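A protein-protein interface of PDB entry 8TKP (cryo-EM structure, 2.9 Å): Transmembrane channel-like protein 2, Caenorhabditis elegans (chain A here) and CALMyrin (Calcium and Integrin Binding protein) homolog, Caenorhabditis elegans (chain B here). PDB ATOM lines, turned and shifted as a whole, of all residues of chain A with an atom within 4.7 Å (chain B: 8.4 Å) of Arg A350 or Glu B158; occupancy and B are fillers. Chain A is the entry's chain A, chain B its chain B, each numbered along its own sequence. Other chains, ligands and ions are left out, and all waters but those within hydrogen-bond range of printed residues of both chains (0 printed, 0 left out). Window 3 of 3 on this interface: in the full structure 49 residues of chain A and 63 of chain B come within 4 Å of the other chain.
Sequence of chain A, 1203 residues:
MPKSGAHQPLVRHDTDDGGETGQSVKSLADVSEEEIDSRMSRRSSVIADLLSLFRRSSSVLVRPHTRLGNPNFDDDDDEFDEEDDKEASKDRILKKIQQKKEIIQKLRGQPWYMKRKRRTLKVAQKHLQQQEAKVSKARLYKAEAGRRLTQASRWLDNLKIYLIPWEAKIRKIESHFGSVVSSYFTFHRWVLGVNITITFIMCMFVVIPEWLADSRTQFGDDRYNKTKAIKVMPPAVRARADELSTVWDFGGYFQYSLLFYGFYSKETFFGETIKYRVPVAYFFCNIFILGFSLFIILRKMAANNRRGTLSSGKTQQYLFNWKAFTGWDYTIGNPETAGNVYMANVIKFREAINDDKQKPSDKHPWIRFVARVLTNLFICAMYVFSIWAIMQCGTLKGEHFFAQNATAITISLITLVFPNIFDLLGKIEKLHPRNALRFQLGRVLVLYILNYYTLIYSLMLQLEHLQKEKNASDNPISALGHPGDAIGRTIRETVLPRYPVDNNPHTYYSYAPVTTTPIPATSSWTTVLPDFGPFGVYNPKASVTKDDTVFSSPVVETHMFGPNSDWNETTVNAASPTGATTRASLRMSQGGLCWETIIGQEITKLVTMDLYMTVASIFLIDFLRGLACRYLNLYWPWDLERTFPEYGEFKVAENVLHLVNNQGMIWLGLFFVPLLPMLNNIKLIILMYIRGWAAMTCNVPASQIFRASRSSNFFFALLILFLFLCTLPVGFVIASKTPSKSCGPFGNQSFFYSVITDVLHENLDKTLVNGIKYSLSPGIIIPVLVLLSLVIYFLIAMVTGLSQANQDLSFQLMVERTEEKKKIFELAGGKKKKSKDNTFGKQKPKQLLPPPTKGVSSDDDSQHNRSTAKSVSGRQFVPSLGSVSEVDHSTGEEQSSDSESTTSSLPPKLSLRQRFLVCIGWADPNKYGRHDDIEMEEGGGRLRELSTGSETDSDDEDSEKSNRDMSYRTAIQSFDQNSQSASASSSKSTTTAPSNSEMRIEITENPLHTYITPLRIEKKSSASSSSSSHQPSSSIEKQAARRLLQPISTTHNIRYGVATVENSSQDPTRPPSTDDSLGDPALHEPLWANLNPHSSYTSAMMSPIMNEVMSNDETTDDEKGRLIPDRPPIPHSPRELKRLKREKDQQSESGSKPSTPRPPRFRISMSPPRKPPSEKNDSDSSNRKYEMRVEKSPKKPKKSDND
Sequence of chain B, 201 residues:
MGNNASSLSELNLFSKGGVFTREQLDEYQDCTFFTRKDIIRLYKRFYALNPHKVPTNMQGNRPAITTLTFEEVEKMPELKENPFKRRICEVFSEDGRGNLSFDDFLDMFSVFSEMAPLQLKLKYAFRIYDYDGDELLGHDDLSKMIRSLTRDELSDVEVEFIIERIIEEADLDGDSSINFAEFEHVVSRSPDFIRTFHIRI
Printed residues of chain B that touch a printed residue of chain A: Thr B150, Glu B153, Leu B154, Glu B158, Phe B161 and Ile B162.
Among the printed residues, pairs that only touch across the chains: Val A346 with Glu B153 (3.3 Å), Arg A350 with Leu B154 (3.4 Å), Phe A349 with Ile B162 (3.5 Å), Ile A353 with Phe B161 (3.6 Å), Ile A353 with Glu B158 (3.7 Å), Val A346 with Thr B150 (3.7 Å), Val A346 with Leu B154 (3.7 Å), Ile A353 with Ile B162 (3.7 Å), Phe A349 with Leu B154 (3.8 Å), Phe A349 with Thr B150 (3.8 Å) and Arg A350 with Glu B153 (3.9 Å).
The guanidinium group (NE) of Arg A350 is in salt-bridge range of the side-chain carboxylate (OE2) of Glu B158 (3.4 Å).
O of Arg A350 lies within hydrogen-bond range of ND2 of Asn A354, 2.6 Å away. The backbone carbonyl oxygen (O) of Ile B146 lies within hydrogen-bond range of the side-chain hydroxyl (OG1) of Thr B150 (2.8 Å). OE1 of Glu B158 is in hydrogen-bond range of N of Ser B155.
Arg A350 touches just these residues of chain B: Glu B153, Leu B154 and Glu B158. Printed residues of chain A within 4 Å of Glu B158: Arg A350 and Ile A353. Printed residues of chain A within 4 Å of Thr B150: Val A346 (3.7 Å) and Phe A349 (3.8 Å). Of the printed residues of chain A, Phe B161 touches Ile A353 (3.6 Å). Of the printed residues of chain A, Ile B162 touches Phe A349 and Ile A353. Printed residues of chain A within 4 Å of Glu B153: Val A346 (3.3 Å) and Arg A350 (3.9 Å). Glu A351 touches none of the printed residues of chain B. The nearest printed residue of chain A that does not touch Ile B162 is Arg A350 (5.8 Å).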
ATOM      1  N   VAL A 346      -8.811 -28.830  -0.087  1.00  0.00           N
ATOM      2  CA  VAL A 346      -8.012 -28.090   0.889  1.00  0.00           C
ATOM      3  C   VAL A 346      -6.576 -28.597   0.881  1.00  0.00           C
ATOM      4  O   VAL A 346      -5.616 -27.813   0.833  1.00  0.00           O
ATOM      5  CB  VAL A 346      -8.637 -28.198   2.290  1.00  0.00           C
ATOM      6  CG1 VAL A 346      -7.680 -27.661   3.340  1.00  0.00           C
ATOM      7  CG2 VAL A 346      -9.956 -27.452   2.341  1.00  0.00           C
ATOM      8  N   ILE A 347      -6.412 -29.921   0.910  1.00  0.00           N
ATOM      9  CA  ILE A 347      -5.077 -30.514   0.925  1.00  0.00           C
ATOM     10  C   ILE A 347      -4.313 -30.142  -0.339  1.00  0.00           C
ATOM     11  O   ILE A 347      -3.137 -29.767  -0.286  1.00  0.00           O
ATOM     12  CB  ILE A 347      -5.171 -32.040   1.100  1.00  0.00           C
ATOM     13  CG1 ILE A 347      -5.690 -32.386   2.497  1.00  0.00           C
ATOM     14  CG2 ILE A 347      -3.821 -32.694   0.854  1.00  0.00           C
ATOM     15  CD1 ILE A 347      -5.787 -33.873   2.757  1.00  0.00           C
ATOM     16  N   LYS A 348      -4.973 -30.239  -1.495  1.00  0.00           N
ATOM     17  CA  LYS A 348      -4.305 -29.963  -2.762  1.00  0.00           C
ATOM     18  C   LYS A 348      -3.864 -28.509  -2.852  1.00  0.00           C
ATOM     19  O   LYS A 348      -2.738 -28.216  -3.266  1.00  0.00           O
ATOM     20  CB  LYS A 348      -5.223 -30.317  -3.931  1.00  0.00           C
ATOM     21  CG  LYS A 348      -5.419 -31.805  -4.147  1.00  0.00           C
ATOM     22  CD  LYS A 348      -6.341 -32.070  -5.323  1.00  0.00           C
ATOM     23  CE  LYS A 348      -6.558 -33.558  -5.533  1.00  0.00           C
ATOM     24  NZ  LYS A 348      -7.479 -33.830  -6.669  1.00  0.00           N
ATOM     25  N   PHE A 349      -4.744 -27.579  -2.473  1.00  0.00           N
ATOM     26  CA  PHE A 349      -4.383 -26.167  -2.537  1.00  0.00           C
ATOM     27  C   PHE A 349      -3.254 -25.840  -1.570  1.00  0.00           C
ATOM     28  O   PHE A 349      -2.312 -25.121  -1.925  1.00  0.00           O
ATOM     29  CB  PHE A 349      -5.604 -25.292  -2.260  1.00  0.00           C
ATOM     30  CG  PHE A 349      -6.507 -25.121  -3.446  1.00  0.00           C
ATOM     31  CD1 PHE A 349      -6.041 -24.527  -4.605  1.00  0.00           C
ATOM     32  CD2 PHE A 349      -7.823 -25.547  -3.401  1.00  0.00           C
ATOM     33  CE1 PHE A 349      -6.864 -24.367  -5.698  1.00  0.00           C
ATOM     34  CE2 PHE A 349      -8.653 -25.389  -4.493  1.00  0.00           C
ATOM     35  CZ  PHE A 349      -8.174 -24.796  -5.642  1.00  0.00           C
ATOM     36  N   ARG A 350      -3.325 -26.363  -0.341  1.00  0.00           N
ATOM     37  CA  ARG A 350      -2.268 -26.093   0.626  1.00  0.00           C
ATOM     38  C   ARG A 350      -0.937 -26.671   0.160  1.00  0.00           C
ATOM     39  O   ARG A 350       0.111 -26.027   0.292  1.00  0.00           O
ATOM     40  CB  ARG A 350      -2.661 -26.654   1.992  1.00  0.00           C
ATOM     41  CG  ARG A 350      -1.858 -26.098   3.149  1.00  0.00           C
ATOM     42  CD  ARG A 350      -2.599 -26.307   4.455  1.00  0.00           C
ATOM     43  NE  ARG A 350      -3.867 -25.588   4.473  1.00  0.00           N
ATOM     44  CZ  ARG A 350      -4.799 -25.736   5.404  1.00  0.00           C
ATOM     45  NH1 ARG A 350      -4.647 -26.585   6.407  1.00  0.00           N
ATOM     46  NH2 ARG A 350      -5.915 -25.015   5.325  1.00  0.00           N
ATOM     47  N   GLU A 351      -0.962 -27.881  -0.402  1.00  0.00           N
ATOM     48  CA  GLU A 351       0.255 -28.486  -0.929  1.00  0.00           C
ATOM     49  C   GLU A 351       0.827 -27.662  -2.075  1.00  0.00           C
ATOM     50  O   GLU A 351       2.030 -27.381  -2.110  1.00  0.00           O
ATOM     51  CB  GLU A 351      -0.037 -29.916  -1.384  1.00  0.00           C
ATOM     52  CG  GLU A 351       0.946 -30.462  -2.403  1.00  0.00           C
ATOM     53  CD  GLU A 351       0.577 -31.854  -2.877  1.00  0.00           C
ATOM     54  OE1 GLU A 351       0.058 -32.644  -2.061  1.00  0.00           O
ATOM     55  OE2 GLU A 351       0.802 -32.156  -4.068  1.00  0.00           O
ATOM     56  N   ALA A 352      -0.027 -27.248  -3.015  1.00  0.00           N
ATOM     57  CA  ALA A 352       0.442 -26.461  -4.150  1.00  0.00           C
ATOM     58  C   ALA A 352       1.043 -25.141  -3.692  1.00  0.00           C
ATOM     59  O   ALA A 352       2.028 -24.664  -4.269  1.00  0.00           O
ATOM     60  CB  ALA A 352      -0.703 -26.219  -5.131  1.00  0.00           C
ATOM     61  N   ILE A 353       0.460 -24.531  -2.660  1.00  0.00           N
ATOM     62  CA  ILE A 353       1.056 -23.333  -2.077  1.00  0.00           C
ATOM     63  C   ILE A 353       2.425 -23.658  -1.491  1.00  0.00           C
ATOM     64  O   ILE A 353       3.394 -22.911  -1.677  1.00  0.00           O
ATOM     65  CB  ILE A 353       0.118 -22.724  -1.021  1.00  0.00           C
ATOM     66  CG1 ILE A 353      -1.137 -22.162  -1.689  1.00  0.00           C
ATOM     67  CG2 ILE A 353       0.834 -21.644  -0.225  1.00  0.00           C
ATOM     68  CD1 ILE A 353      -2.126 -21.563  -0.718  1.00  0.00           C
ATOM     69  N   ASN A 354       2.529 -24.781  -0.785  1.00  0.00           N
ATOM     70  CA  ASN A 354       3.765 -25.152  -0.109  1.00  0.00           C
ATOM     71  C   ASN A 354       4.687 -26.025  -0.955  1.00  0.00           C
ATOM     72  O   ASN A 354       5.754 -26.413  -0.471  1.00  0.00           O
ATOM     73  CB  ASN A 354       3.449 -25.865   1.207  1.00  0.00           C
ATOM     74  CG  ASN A 354       2.788 -24.950   2.218  1.00  0.00           C
ATOM     75  OD1 ASN A 354       3.464 -24.298   3.014  1.00  0.00           O
ATOM     76  ND2 ASN A 354       1.462 -24.893   2.190  1.00  0.00           N
ATOM     77  N   ILE B 146     -13.312 -19.971  -4.356  1.00  0.00           N
ATOM     78  CA  ILE B 146     -12.386 -20.722  -3.513  1.00  0.00           C
ATOM     79  C   ILE B 146     -13.009 -21.003  -2.152  1.00  0.00           C
ATOM     80  O   ILE B 146     -12.882 -22.109  -1.609  1.00  0.00           O
ATOM     81  CB  ILE B 146     -11.051 -19.965  -3.380  1.00  0.00           C
ATOM     82  CG1 ILE B 146     -10.333 -19.918  -4.728  1.00  0.00           C
ATOM     83  CG2 ILE B 146     -10.168 -20.613  -2.328  1.00  0.00           C
ATOM     84  CD1 ILE B 146      -9.081 -19.077  -4.716  1.00  0.00           C
ATOM     85  N   ARG B 147     -13.690 -20.006  -1.577  1.00  0.00           N
ATOM     86  CA  ARG B 147     -14.363 -20.209  -0.297  1.00  0.00           C
ATOM     87  C   ARG B 147     -15.359 -21.358  -0.383  1.00  0.00           C
ATOM     88  O   ARG B 147     -15.408 -22.223   0.499  1.00  0.00           O
ATOM     89  CB  ARG B 147     -15.078 -18.929   0.142  1.00  0.00           C
ATOM     90  CG  ARG B 147     -14.192 -17.712   0.328  1.00  0.00           C
ATOM     91  CD  ARG B 147     -13.058 -17.966   1.300  1.00  0.00           C
ATOM     92  NE  ARG B 147     -12.794 -16.796   2.130  1.00  0.00           N
ATOM     93  CZ  ARG B 147     -12.160 -15.706   1.718  1.00  0.00           C
ATOM     94  NH1 ARG B 147     -11.715 -15.593   0.477  1.00  0.00           N
ATOM     95  NH2 ARG B 147     -11.974 -14.703   2.569  1.00  0.00           N
ATOM     96  N   THR B 150     -13.505 -24.843  -0.780  1.00  0.00           N
ATOM     97  CA  THR B 150     -12.762 -25.346   0.369  1.00  0.00           C
ATOM     98  C   THR B 150     -13.519 -25.162   1.678  1.00  0.00           C
ATOM     99  O   THR B 150     -12.938 -25.342   2.753  1.00  0.00           O
ATOM    100  CB  THR B 150     -11.392 -24.674   0.454  1.00  0.00           C
ATOM    101  OG1 THR B 150     -11.559 -23.254   0.547  1.00  0.00           O
ATOM    102  CG2 THR B 150     -10.568 -25.002  -0.779  1.00  0.00           C
ATOM    103  N   ASP B 152     -14.360 -22.591   3.198  1.00  0.00           N
ATOM    104  CA  ASP B 152     -13.722 -21.505   3.936  1.00  0.00           C
ATOM    105  C   ASP B 152     -12.635 -21.993   4.888  1.00  0.00           C
ATOM    106  O   ASP B 152     -12.237 -21.250   5.793  1.00  0.00           O
ATOM    107  CB  ASP B 152     -14.754 -20.673   4.710  1.00  0.00           C
ATOM    108  CG  ASP B 152     -15.902 -20.211   3.837  1.00  0.00           C
ATOM    109  OD1 ASP B 152     -16.736 -21.058   3.451  1.00  0.00           O
ATOM    110  OD2 ASP B 152     -15.971 -19.001   3.535  1.00  0.00           O
ATOM    111  N   GLU B 153     -12.142 -23.220   4.712  1.00  0.00           N
ATOM    112  CA  GLU B 153     -11.115 -23.736   5.609  1.00  0.00           C
ATOM    113  C   GLU B 153      -9.777 -23.045   5.378  1.00  0.00           C
ATOM    114  O   GLU B 153      -9.024 -22.801   6.326  1.00  0.00           O
ATOM    115  CB  GLU B 153     -10.980 -25.248   5.447  1.00  0.00           C
ATOM    116  CG  GLU B 153     -12.159 -26.032   5.999  1.00  0.00           C
ATOM    117  CD  GLU B 153     -11.913 -27.527   6.013  1.00  0.00           C
ATOM    118  OE1 GLU B 153     -10.907 -27.973   5.424  1.00  0.00           O
ATOM    119  OE2 GLU B 153     -12.726 -28.258   6.617  1.00  0.00           O
ATOM    120  N   LEU B 154      -9.461 -22.730   4.123  1.00  0.00           N
ATOM    121  CA  LEU B 154      -8.212 -22.042   3.824  1.00  0.00           C
ATOM    122  C   LEU B 154      -8.217 -20.643   4.428  1.00  0.00           C
ATOM    123  O   LEU B 154      -9.259 -19.992   4.544  1.00  0.00           O
ATOM    124  CB  LEU B 154      -7.996 -21.960   2.313  1.00  0.00           C
ATOM    125  CG  LEU B 154      -7.923 -23.284   1.552  1.00  0.00           C
ATOM    126  CD1 LEU B 154      -7.607 -23.039   0.086  1.00  0.00           C
ATOM    127  CD2 LEU B 154      -6.896 -24.208   2.178  1.00  0.00           C
ATOM    128  N   SER B 155      -7.033 -20.182   4.820  1.00  0.00           N
ATOM    129  CA  SER B 155      -6.898 -18.859   5.405  1.00  0.00           C
ATOM    130  C   SER B 155      -6.976 -17.785   4.320  1.00  0.00           C
ATOM    131  O   SER B 155      -6.893 -18.063   3.122  1.00  0.00           O
ATOM    132  CB  SER B 155      -5.586 -18.745   6.177  1.00  0.00           C
ATOM    133  OG  SER B 155      -4.473 -18.904   5.315  1.00  0.00           O
ATOM    134  N   ASP B 156      -7.140 -16.537   4.765  1.00  0.00           N
ATOM    135  CA  ASP B 156      -7.289 -15.431   3.824  1.00  0.00           C
ATOM    136  C   ASP B 156      -6.038 -15.251   2.972  1.00  0.00           C
ATOM    137  O   ASP B 156      -6.132 -15.008   1.762  1.00  0.00           O
ATOM    138  CB  ASP B 156      -7.612 -14.141   4.581  1.00  0.00           C
ATOM    139  CG  ASP B 156      -8.877 -14.256   5.408  1.00  0.00           C
ATOM    140  OD1 ASP B 156      -9.756 -15.065   5.043  1.00  0.00           O
ATOM    141  OD2 ASP B 156      -8.993 -13.534   6.420  1.00  0.00           O
ATOM    142  N   VAL B 157      -4.857 -15.362   3.585  1.00  0.00           N
ATOM    143  CA  VAL B 157      -3.614 -15.195   2.837  1.00  0.00           C
ATOM    144  C   VAL B 157      -3.473 -16.287   1.783  1.00  0.00           C
ATOM    145  O   VAL B 157      -3.034 -16.030   0.656  1.00  0.00           O
ATOM    146  CB  VAL B 157      -2.411 -15.161   3.799  1.00  0.00           C
ATOM    147  CG1 VAL B 157      -2.470 -16.323   4.779  1.00  0.00           C
ATOM    148  CG2 VAL B 157      -1.101 -15.172   3.023  1.00  0.00           C
ATOM    149  N   GLU B 158      -3.848 -17.521   2.131  1.00  0.00           N
ATOM    150  CA  GLU B 158      -3.800 -18.609   1.160  1.00  0.00           C
ATOM    151  C   GLU B 158      -4.732 -18.341  -0.014  1.00  0.00           C
ATOM    152  O   GLU B 158      -4.361 -18.558  -1.175  1.00  0.00           O
ATOM    153  CB  GLU B 158      -4.164 -19.931   1.836  1.00  0.00           C
ATOM    154  CG  GLU B 158      -3.133 -20.427   2.835  1.00  0.00           C
ATOM    155  CD  GLU B 158      -3.662 -21.551   3.702  1.00  0.00           C
ATOM    156  OE1 GLU B 158      -4.895 -21.626   3.889  1.00  0.00           O
ATOM    157  OE2 GLU B 158      -2.849 -22.359   4.198  1.00  0.00           O
ATOM    158  N   VAL B 159      -5.946 -17.865   0.267  1.00  0.00           N
ATOM    159  CA  VAL B 159      -6.897 -17.571  -0.801  1.00  0.00           C
ATOM    160  C   VAL B 159      -6.363 -16.464  -1.697  1.00  0.00           C
ATOM    161  O   VAL B 159      -6.455 -16.543  -2.928  1.00  0.00           O
ATOM    162  CB  VAL B 159      -8.272 -17.209  -0.211  1.00  0.00           C
ATOM    163  CG1 VAL B 159      -9.224 -16.783  -1.315  1.00  0.00           C
ATOM    164  CG2 VAL B 159      -8.844 -18.387   0.558  1.00  0.00           C
ATOM    165  N   GLU B 160      -5.803 -15.411  -1.096  1.00  0.00           N
ATOM    166  CA  GLU B 160      -5.241 -14.325  -1.893  1.00  0.00           C
ATOM    167  C   GLU B 160      -4.096 -14.819  -2.766  1.00  0.00           C
ATOM    168  O   GLU B 160      -3.992 -14.439  -3.939  1.00  0.00           O
ATOM    169  CB  GLU B 160      -4.771 -13.190  -0.982  1.00  0.00           C
ATOM    170  CG  GLU B 160      -5.884 -12.511  -0.202  1.00  0.00           C
ATOM    171  CD  GLU B 160      -6.852 -11.756  -1.091  1.00  0.00           C
ATOM    172  OE1 GLU B 160      -6.462 -11.375  -2.216  1.00  0.00           O
ATOM    173  OE2 GLU B 160      -8.007 -11.542  -0.665  1.00  0.00           O
ATOM    174  N   PHE B 161      -3.228 -15.668  -2.214  1.00  0.00           N
ATOM    175  CA  PHE B 161      -2.127 -16.215  -2.997  1.00  0.00           C
ATOM    176  C   PHE B 161      -2.642 -17.044  -4.166  1.00  0.00           C
ATOM    177  O   PHE B 161      -2.122 -16.944  -5.284  1.00  0.00           O
ATOM    178  CB  PHE B 161      -1.215 -17.054  -2.102  1.00  0.00           C
ATOM    179  CG  PHE B 161      -0.089 -17.719  -2.839  1.00  0.00           C
ATOM    180  CD1 PHE B 161       1.067 -17.018  -3.138  1.00  0.00           C
ATOM    181  CD2 PHE B 161      -0.185 -19.042  -3.231  1.00  0.00           C
ATOM    182  CE1 PHE B 161       2.105 -17.627  -3.816  1.00  0.00           C
ATOM    183  CE2 PHE B 161       0.850 -19.656  -3.909  1.00  0.00           C
ATOM    184  CZ  PHE B 161       1.996 -18.947  -4.202  1.00  0.00           C
ATOM    185  N   ILE B 162      -3.662 -17.871  -3.927  1.00  0.00           N
ATOM    186  CA  ILE B 162      -4.207 -18.699  -5.000  1.00  0.00           C
ATOM    187  C   ILE B 162      -4.835 -17.828  -6.081  1.00  0.00           C
ATOM    188  O   ILE B 162      -4.673 -18.089  -7.280  1.00  0.00           O
ATOM    189  CB  ILE B 162      -5.213 -19.718  -4.436  1.00  0.00           C
ATOM    190  CG1 ILE B 162      -4.518 -20.659  -3.453  1.00  0.00           C
ATOM    191  CG2 ILE B 162      -5.842 -20.522  -5.559  1.00  0.00           C
ATOM    192  CD1 ILE B 162      -5.464 -21.577  -2.719  1.00  0.00           C
ATOM    193  N   ILE B 163      -5.560 -16.782  -5.678  1.00  0.00           N
ATOM    194  CA  ILE B 163      -6.159 -15.870  -6.651  1.00  0.00           C
ATOM    195  C   ILE B 163      -5.078 -15.201  -7.486  1.00  0.00           C
ATOM    196  O   ILE B 163      -5.199 -15.090  -8.713  1.00  0.00           O
ATOM    197  CB  ILE B 163      -7.037 -14.825  -5.940  1.00  0.00           C
ATOM    198  CG1 ILE B 163      -8.231 -15.488  -5.260  1.00  0.00           C
ATOM    199  CG2 ILE B 163      -7.515 -13.772  -6.924  1.00  0.00           C
ATOM    200  CD1 ILE B 163      -8.932 -14.573  -4.292  1.00  0.00           C
ATOM    201  N   GLU B 164      -4.010 -14.735  -6.834  1.00  0.00           N
ATOM    202  CA  GLU B 164      -2.928 -14.082  -7.560  1.00  0.00           C
ATOM    203  C   GLU B 164      -2.264 -15.043  -8.536  1.00  0.00           C
ATOM    204  O   GLU B 164      -1.946 -14.665  -9.668  1.00  0.00           O
ATOM    205  CB  GLU B 164      -1.901 -13.519  -6.577  1.00  0.00           C
ATOM    206  CG  GLU B 164      -2.420 -12.365  -5.737  1.00  0.00           C
ATOM    207  CD  GLU B 164      -1.454 -11.965  -4.641  1.00  0.00           C
ATOM    208  OE1 GLU B 164      -0.365 -12.570  -4.557  1.00  0.00           O
ATOM    209  OE2 GLU B 164      -1.785 -11.047  -3.861  1.00  0.00           O
ATOM    210  N   ARG B 165      -2.049 -16.291  -8.117  1.00  0.00           N
ATOM    211  CA  ARG B 165      -1.451 -17.274  -9.016  1.00  0.00           C
ATOM    212  C   ARG B 165      -2.357 -17.554 -10.209  1.00  0.00           C
ATOM    213  O   ARG B 165      -1.883 -17.645 -11.347  1.00  0.00           O
ATOM    214  CB  ARG B 165      -1.149 -18.566  -8.258  1.00  0.00           C
ATOM    215  CG  ARG B 165      -0.050 -18.427  -7.220  1.00  0.00           C
ATOM    216  CD  ARG B 165       1.242 -17.940  -7.852  1.00  0.00           C
ATOM    217  NE  ARG B 165       1.693 -18.832  -8.915  1.00  0.00           N
ATOM    218  CZ  ARG B 165       2.443 -19.907  -8.721  1.00  0.00           C
ATOM    219  NH1 ARG B 165       2.846 -20.261  -7.511  1.00  0.00           N
ATOM    220  NH2 ARG B 165       2.796 -20.648  -9.767  1.00  0.00           N
